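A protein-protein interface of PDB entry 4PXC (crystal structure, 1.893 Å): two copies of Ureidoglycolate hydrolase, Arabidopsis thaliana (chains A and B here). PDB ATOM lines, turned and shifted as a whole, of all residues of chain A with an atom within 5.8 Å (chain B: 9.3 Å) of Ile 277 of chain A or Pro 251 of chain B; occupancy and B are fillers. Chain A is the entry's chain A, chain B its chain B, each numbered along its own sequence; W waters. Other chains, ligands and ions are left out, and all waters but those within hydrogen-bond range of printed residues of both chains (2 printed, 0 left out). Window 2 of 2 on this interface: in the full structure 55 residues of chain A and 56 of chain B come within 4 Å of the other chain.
Among the printed residues, pairs that only touch across the chains: Ile 277 of chain A with Pro 251 of chain B, Arg 375 of chain A with Gly 246 of chain B, Ile 277 of chain A with Leu 249 of chain B, Val 280 of chain A with Gly 246 of chain B, Arg 375 of chain A with Ala 247 of chain B, Thr 279 of chain A with Met 250 of chain B, Arg 375 of chain A with Leu 249 of chain B, Val 280 of chain A with Arg 253 of chain B and Val 280 of chain A with Val 248 of chain B.
No position is printed for both chains.
Of the 9 pairs that touch across the chains among the printed residues, none has its exchanged pair printed and touching as well.
The side-chain hydroxyl (OG) of Ser 274 of chain A lies within hydrogen-bond range of the side-chain hydroxyl (OG1) of Thr 279 of chain A (2.6 Å).
OG1 of Thr 279 of chain A lies within hydrogen-bond range of O of Ser 276 of chain A, 3.4 Å away.
The guanidinium group (NH1) of Arg 375 of chain A lies within salt-bridge range of the side-chain carboxylate (OD1) of Asp 278 of chain A (2.9 Å).
The backbone carbonyl oxygen of Val 248 of chain B sits at hydrogen-bond distance from the guanidinium group of Arg 253 of chain B, at 2.9 Å.
Water W1 lies within hydrogen-bond range of the backbone carbonyl oxygen (O) of Ile 277 of chain A (2.5 Å), the backbone carbonyl oxygen (O) of Thr 279 of chain A (2.7 Å) and the backbone NH (N) of Met 250 of chain B (3.1 Å).
Water W2 lies within hydrogen-bond range of the backbone carbonyl oxygen (O) of Gly 246 of chain B (2.8 Å) and the backbone carbonyl oxygen (O) of Arg 375 of chain A (2.9 Å).
Of chain B, only Leu 249 and Pro 251 come within 4 Å of Ile 277 of chain A.
Of the printed residues of chain A, Pro 251 of chain B touches Ile 277.
No residue of chain B comes within 4 Å of Ser 276 of chain A.
Of the printed residues of chain A, Leu 249 of chain B touches Ile 277 and Arg 375.
Printed residues of chain A within 4 Å of Ala 247 of chain B: Arg 375 (3.7 Å).
Of the printed residues of chain A, Arg 253 of chain B touches Val 280 (3.8 Å).
Of the printed residues of chain A, Val 248 of chain B touches Val 280 (3.8 Å).
Asp 255 of chain B touches none of the printed residues of chain A.
The nearest printed residue of chain A that does not touch Pro 251 of chain B is Thr 279 of chain A (6.7 Å).
The nearest printed residue of chain A that does not touch Met 250 of chain B is Val 280 of chain A (4.2 Å).
Hydrophobic or aromatic side chains of chain B within 4 Å of the printed part of chain A: Leu 249, Met 250 and Pro 251.
Of the 8 printed residues of chain A, 4 touch a printed residue of chain B.
Hydrophobic or aromatic side chains of chain A that line the printed part of chain B: Ile 277 and Val 280.
Among the printed residues, no Asp or Glu carboxylate lies within 4 Å of a Lys or Arg side-chain nitrogen of the other chain.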
ATOM      1  N   SER A 274      24.874  14.339  10.659  1.00  0.00           N
ATOM      2  CA  SER A 274      23.964  15.464  10.860  1.00  0.00           C
ATOM      3  C   SER A 274      22.547  15.105  10.440  1.00  0.00           C
ATOM      4  O   SER A 274      21.591  15.806  10.784  1.00  0.00           O
ATOM      5  CB  SER A 274      24.417  16.680  10.050  1.00  0.00           C
ATOM      6  OG  SER A 274      23.935  16.575   8.720  1.00  0.00           O
ATOM      7  N   GLU A 275      22.427  14.030   9.672  1.00  0.00           N
ATOM      8  CA  GLU A 275      21.137  13.568   9.139  1.00  0.00           C
ATOM      9  C   GLU A 275      20.488  14.551   8.160  1.00  0.00           C
ATOM     10  O   GLU A 275      19.335  14.356   7.754  1.00  0.00           O
ATOM     11  CB  GLU A 275      20.165  13.203  10.268  1.00  0.00           C
ATOM     12  CG  GLU A 275      20.675  12.095  11.191  1.00  0.00           C
ATOM     13  CD  GLU A 275      20.843  10.766  10.467  1.00  0.00           C
ATOM     14  OE1 GLU A 275      19.875   9.970  10.459  1.00  0.00           O
ATOM     15  OE2 GLU A 275      21.939  10.514   9.908  1.00  0.00           O
ATOM     16  N   SER A 276      21.229  15.589   7.771  1.00  0.00           N
ATOM     17  CA  SER A 276      20.733  16.545   6.780  1.00  0.00           C
ATOM     18  C   SER A 276      21.567  16.555   5.506  1.00  0.00           C
ATOM     19  O   SER A 276      22.804  16.589   5.556  1.00  0.00           O
ATOM     20  CB  SER A 276      20.684  17.959   7.348  1.00  0.00           C
ATOM     21  OG  SER A 276      20.364  18.880   6.308  1.00  0.00           O
ATOM     22  N   ILE A 277      20.878  16.537   4.367  1.00  0.00           N
ATOM     23  CA  ILE A 277      21.527  16.652   3.065  1.00  0.00           C
ATOM     24  C   ILE A 277      22.256  17.994   2.890  1.00  0.00           C
ATOM     25  O   ILE A 277      23.179  18.097   2.081  1.00  0.00           O
ATOM     26  CB  ILE A 277      20.502  16.440   1.916  1.00  0.00           C
ATOM     27  CG1 ILE A 277      21.205  16.233   0.578  1.00  0.00           C
ATOM     28  CG2 ILE A 277      19.512  17.597   1.835  1.00  0.00           C
ATOM     29  CD1 ILE A 277      21.803  14.881   0.432  1.00  0.00           C
ATOM     30  N   ASP A 278      21.869  19.012   3.660  1.00  0.00           N
ATOM     31  CA  ASP A 278      22.450  20.358   3.496  1.00  0.00           C
ATOM     32  C   ASP A 278      23.833  20.544   4.125  1.00  0.00           C
ATOM     33  O   ASP A 278      24.482  21.581   3.928  1.00  0.00           O
ATOM     34  CB  ASP A 278      21.492  21.416   4.034  1.00  0.00           C
ATOM     35  CG  ASP A 278      20.222  21.500   3.221  1.00  0.00           C
ATOM     36  OD1 ASP A 278      20.321  21.451   1.974  1.00  0.00           O
ATOM     37  OD2 ASP A 278      19.135  21.588   3.827  1.00  0.00           O
ATOM     38  N   THR A 279      24.284  19.544   4.874  1.00  0.00           N
ATOM     39  CA  THR A 279      25.581  19.612   5.534  1.00  0.00           C
ATOM     40  C   THR A 279      26.672  19.100   4.605  1.00  0.00           C
ATOM     41  O   THR A 279      26.529  18.046   3.995  1.00  0.00           O
ATOM     42  CB  THR A 279      25.599  18.727   6.803  1.00  0.00           C
ATOM     43  OG1 THR A 279      24.375  18.894   7.533  1.00  0.00           O
ATOM     44  CG2 THR A 279      26.785  19.093   7.694  1.00  0.00           C
ATOM     45  N   VAL A 280      27.772  19.843   4.505  1.00  0.00           N
ATOM     46  CA  VAL A 280      28.937  19.367   3.767  1.00  0.00           C
ATOM     47  C   VAL A 280      30.210  19.539   4.603  1.00  0.00           C
ATOM     48  O   VAL A 280      30.259  20.358   5.523  1.00  0.00           O
ATOM     49  CB  VAL A 280      29.094  20.098   2.412  1.00  0.00           C
ATOM     50  CG1 VAL A 280      27.912  19.786   1.490  1.00  0.00           C
ATOM     51  CG2 VAL A 280      29.221  21.614   2.634  1.00  0.00           C
ATOM     52  N   ARG A 375      24.673  27.644  -1.578  1.00  0.00           N
ATOM     53  CA  ARG A 375      25.458  26.740  -0.737  1.00  0.00           C
ATOM     54  C   ARG A 375      26.889  27.253  -0.610  1.00  0.00           C
ATOM     55  O   ARG A 375      27.499  27.164   0.454  1.00  0.00           O
ATOM     56  CB  ARG A 375      25.460  25.325  -1.306  1.00  0.00           C
ATOM     57  CG  ARG A 375      24.071  24.760  -1.543  1.00  0.00           C
ATOM     58  CD  ARG A 375      24.140  23.286  -1.916  1.00  0.00           C
ATOM     59  NE  ARG A 375      22.806  22.717  -2.118  1.00  0.00           N
ATOM     60  CZ  ARG A 375      21.963  22.398  -1.139  1.00  0.00           C
ATOM     61  NH1 ARG A 375      22.296  22.596   0.128  1.00  0.00           N
ATOM     62  NH2 ARG A 375      20.774  21.882  -1.430  1.00  0.00           N
ATOM     63  N   GLY B 246      31.753  23.357  -1.194  1.00  0.00           N
ATOM     64  CA  GLY B 246      30.581  23.848  -0.485  1.00  0.00           C
ATOM     65  C   GLY B 246      29.260  23.427  -1.110  1.00  0.00           C
ATOM     66  O   GLY B 246      28.235  23.346  -0.423  1.00  0.00           O
ATOM     67  N   ALA B 247      29.281  23.134  -2.405  1.00  0.00           N
ATOM     68  CA  ALA B 247      28.049  22.958  -3.169  1.00  0.00           C
ATOM     69  C   ALA B 247      27.727  21.520  -3.575  1.00  0.00           C
ATOM     70  O   ALA B 247      26.545  21.171  -3.719  1.00  0.00           O
ATOM     71  CB  ALA B 247      28.055  23.865  -4.393  1.00  0.00           C
ATOM     72  N   VAL B 248      28.753  20.687  -3.778  1.00  0.00           N
ATOM     73  CA  VAL B 248      28.513  19.284  -4.128  1.00  0.00           C
ATOM     74  C   VAL B 248      28.091  18.510  -2.877  1.00  0.00           C
ATOM     75  O   VAL B 248      28.877  18.361  -1.929  1.00  0.00           O
ATOM     76  CB  VAL B 248      29.755  18.619  -4.780  1.00  0.00           C
ATOM     77  CG1 VAL B 248      29.437  17.184  -5.194  1.00  0.00           C
ATOM     78  CG2 VAL B 248      30.219  19.419  -6.001  1.00  0.00           C
ATOM     79  N   LEU B 249      26.854  18.012  -2.872  1.00  0.00           N
ATOM     80  CA  LEU B 249      26.324  17.358  -1.680  1.00  0.00           C
ATOM     81  C   LEU B 249      26.964  15.980  -1.518  1.00  0.00           C
ATOM     82  O   LEU B 249      27.378  15.372  -2.507  1.00  0.00           O
ATOM     83  CB  LEU B 249      24.794  17.281  -1.738  1.00  0.00           C
ATOM     84  CG  LEU B 249      24.106  18.647  -1.905  1.00  0.00           C
ATOM     85  CD1 LEU B 249      22.578  18.525  -1.935  1.00  0.00           C
ATOM     86  CD2 LEU B 249      24.529  19.616  -0.806  1.00  0.00           C
ATOM     87  N   MET B 250      27.065  15.501  -0.277  1.00  0.00           N
ATOM     88  CA  MET B 250      27.820  14.266   0.012  1.00  0.00           C
ATOM     89  C   MET B 250      27.489  13.031  -0.849  1.00  0.00           C
ATOM     90  O   MET B 250      28.411  12.357  -1.328  1.00  0.00           O
ATOM     91  CB  MET B 250      27.780  13.909   1.506  1.00  0.00           C
ATOM     92  CG  MET B 250      28.203  15.050   2.428  1.00  0.00           C
ATOM     93  SD  MET B 250      29.945  15.528   2.323  1.00  0.00           S
ATOM     94  CE  MET B 250      30.725  14.151   3.158  1.00  0.00           C
ATOM     95  N   PRO B 251      26.190  12.733  -1.064  1.00  0.00           N
ATOM     96  CA  PRO B 251      25.874  11.533  -1.853  1.00  0.00           C
ATOM     97  C   PRO B 251      26.471  11.517  -3.261  1.00  0.00           C
ATOM     98  O   PRO B 251      26.601  10.433  -3.833  1.00  0.00           O
ATOM     99  CB  PRO B 251      24.343  11.581  -1.955  1.00  0.00           C
ATOM    100  CG  PRO B 251      23.913  12.338  -0.742  1.00  0.00           C
ATOM    101  CD  PRO B 251      24.966  13.393  -0.564  1.00  0.00           C
ATOM    102  N   TYR B 252      26.819  12.682  -3.810  1.00  0.00           N
ATOM    103  CA  TYR B 252      27.242  12.763  -5.212  1.00  0.00           C
ATOM    104  C   TYR B 252      28.757  12.782  -5.393  1.00  0.00           C
ATOM    105  O   TYR B 252      29.259  12.899  -6.513  1.00  0.00           O
ATOM    106  CB  TYR B 252      26.601  13.989  -5.882  1.00  0.00           C
ATOM    107  CG  TYR B 252      25.102  13.994  -5.723  1.00  0.00           C
ATOM    108  CD1 TYR B 252      24.304  13.171  -6.503  1.00  0.00           C
ATOM    109  CD2 TYR B 252      24.487  14.791  -4.770  1.00  0.00           C
ATOM    110  CE1 TYR B 252      22.933  13.158  -6.353  1.00  0.00           C
ATOM    111  CE2 TYR B 252      23.119  14.785  -4.613  1.00  0.00           C
ATOM    112  CZ  TYR B 252      22.345  13.968  -5.409  1.00  0.00           C
ATOM    113  OH  TYR B 252      20.975  13.960  -5.254  1.00  0.00           O
ATOM    114  N   ARG B 253      29.480  12.626  -4.291  1.00  0.00           N
ATOM    115  CA  ARG B 253      30.932  12.749  -4.319  1.00  0.00           C
ATOM    116  C   ARG B 253      31.668  11.446  -4.631  1.00  0.00           C
ATOM    117  O   ARG B 253      31.154  10.351  -4.406  1.00  0.00           O
ATOM    118  CB  ARG B 253      31.412  13.281  -2.963  1.00  0.00           C
ATOM    119  CG  ARG B 253      30.836  14.644  -2.622  1.00  0.00           C
ATOM    120  CD  ARG B 253      31.449  15.205  -1.358  1.00  0.00           C
ATOM    121  NE  ARG B 253      31.045  16.595  -1.177  1.00  0.00           N
ATOM    122  CZ  ARG B 253      31.716  17.474  -0.448  1.00  0.00           C
ATOM    123  NH1 ARG B 253      32.831  17.099   0.175  1.00  0.00           N
ATOM    124  NH2 ARG B 253      31.285  18.724  -0.349  1.00  0.00           N
ATOM    125  N   ASN B 254      32.878  11.586  -5.158  1.00  0.00           N
ATOM    126  CA  ASN B 254      33.843  10.494  -5.202  1.00  0.00           C
ATOM    127  C   ASN B 254      35.214  11.063  -4.852  1.00  0.00           C
ATOM    128  O   ASN B 254      36.032  11.345  -5.726  1.00  0.00           O
ATOM    129  CB  ASN B 254      33.823   9.731  -6.544  1.00  0.00           C
ATOM    130  CG  ASN B 254      34.119  10.605  -7.758  1.00  0.00           C
ATOM    131  OD1 ASN B 254      33.959  11.825  -7.738  1.00  0.00           O
ATOM    132  ND2 ASN B 254      34.537   9.958  -8.843  1.00  0.00           N
ATOM    133  N   ASP B 255      35.428  11.239  -3.546  1.00  0.00           N
ATOM    134  CA  ASP B 255      36.530  12.026  -2.992  1.00  0.00           C
ATOM    135  C   ASP B 255      37.833  11.230  -3.062  1.00  0.00           C
ATOM    136  O   ASP B 255      37.991  10.206  -2.380  1.00  0.00           O
ATOM    137  CB  ASP B 255      36.189  12.395  -1.530  1.00  0.00           C
ATOM    138  CG  ASP B 255      37.107  13.463  -0.941  1.00  0.00           C
ATOM    139  OD1 ASP B 255      38.340  13.407  -1.165  1.00  0.00           O
ATOM    140  OD2 ASP B 255      36.590  14.363  -0.232  1.00  0.00           O
ATOM    141  N   ILE B 296      37.112  19.858  -3.912  1.00  0.00           N
ATOM    142  CA  ILE B 296      37.157  18.437  -3.580  1.00  0.00           C
ATOM    143  C   ILE B 296      38.252  17.754  -4.388  1.00  0.00           C
ATOM    144  O   ILE B 296      38.291  17.890  -5.613  1.00  0.00           O
ATOM    145  CB  ILE B 296      35.816  17.743  -3.885  1.00  0.00           C
ATOM    146  CG1 ILE B 296      34.663  18.470  -3.172  1.00  0.00           C
ATOM    147  CG2 ILE B 296      35.879  16.270  -3.487  1.00  0.00           C
ATOM    148  CD1 ILE B 296      33.279  18.018  -3.671  1.00  0.00           C
ATOM    149  N   LYS B 331      34.587   1.061  -3.910  1.00  0.00           N
ATOM    150  CA  LYS B 331      33.684   1.561  -2.875  1.00  0.00           C
ATOM    151  C   LYS B 331      33.531   3.079  -2.947  1.00  0.00           C
ATOM    152  O   LYS B 331      32.432   3.607  -2.766  1.00  0.00           O
ATOM    153  CB  LYS B 331      34.159   1.158  -1.483  1.00  0.00           C
ATOM    154  CG  LYS B 331      33.278   1.709  -0.367  1.00  0.00           C
ATOM    155  CD  LYS B 331      32.584   0.588   0.398  1.00  0.00           C
ATOM    156  CE  LYS B 331      31.401   1.109   1.211  1.00  0.00           C
ATOM    157  NZ  LYS B 331      30.757   0.009   1.989  1.00  0.00           N
ATOM    158  N   ARG B 332      34.638   3.773  -3.196  1.00  0.00           N
ATOM    159  CA  ARG B 332      34.631   5.237  -3.271  1.00  0.00           C
ATOM    160  C   ARG B 332      34.145   5.732  -4.632  1.00  0.00           C
ATOM    161  O   ARG B 332      33.908   6.928  -4.815  1.00  0.00           O
ATOM    162  CB  ARG B 332      36.034   5.800  -3.003  1.00  0.00           C
ATOM    163  CG  ARG B 332      36.447   5.832  -1.525  1.00  0.00           C
ATOM    164  CD  ARG B 332      35.843   7.042  -0.813  1.00  0.00           C
ATOM    165  NE  ARG B 332      35.901   6.894   0.642  1.00  0.00           N
ATOM    166  CZ  ARG B 332      35.155   7.584   1.499  1.00  0.00           C
ATOM    167  NH1 ARG B 332      34.282   8.485   1.058  1.00  0.00           N
ATOM    168  NH2 ARG B 332      35.279   7.375   2.801  1.00  0.00           N
ATOM    169  N   LYS B 333      34.021   4.809  -5.577  1.00  0.00           N
ATOM    170  CA  LYS B 333      33.622   5.126  -6.948  1.00  0.00           C
ATOM    171  C   LYS B 333      34.625   6.055  -7.620  1.00  0.00           C
ATOM    172  O   LYS B 333      34.261   6.943  -8.390  1.00  0.00           O
ATOM    173  CB  LYS B 333      32.201   5.696  -6.995  1.00  0.00           C
ATOM    174  CG  LYS B 333      31.187   4.803  -6.273  1.00  0.00           C
ATOM    175  CD  LYS B 333      29.760   5.267  -6.496  1.00  0.00           C
ATOM    176  CE  LYS B 333      29.465   6.544  -5.737  1.00  0.00           C
ATOM    177  NZ  LYS B 333      28.462   6.319  -4.657  1.00  0.00           N
HETATM  178  O   HOH W   1      25.346  16.788   1.944  1.00  0.00           O
HETATM  179  O   HOH W   2      26.960  24.610   1.772  1.00  0.00           O
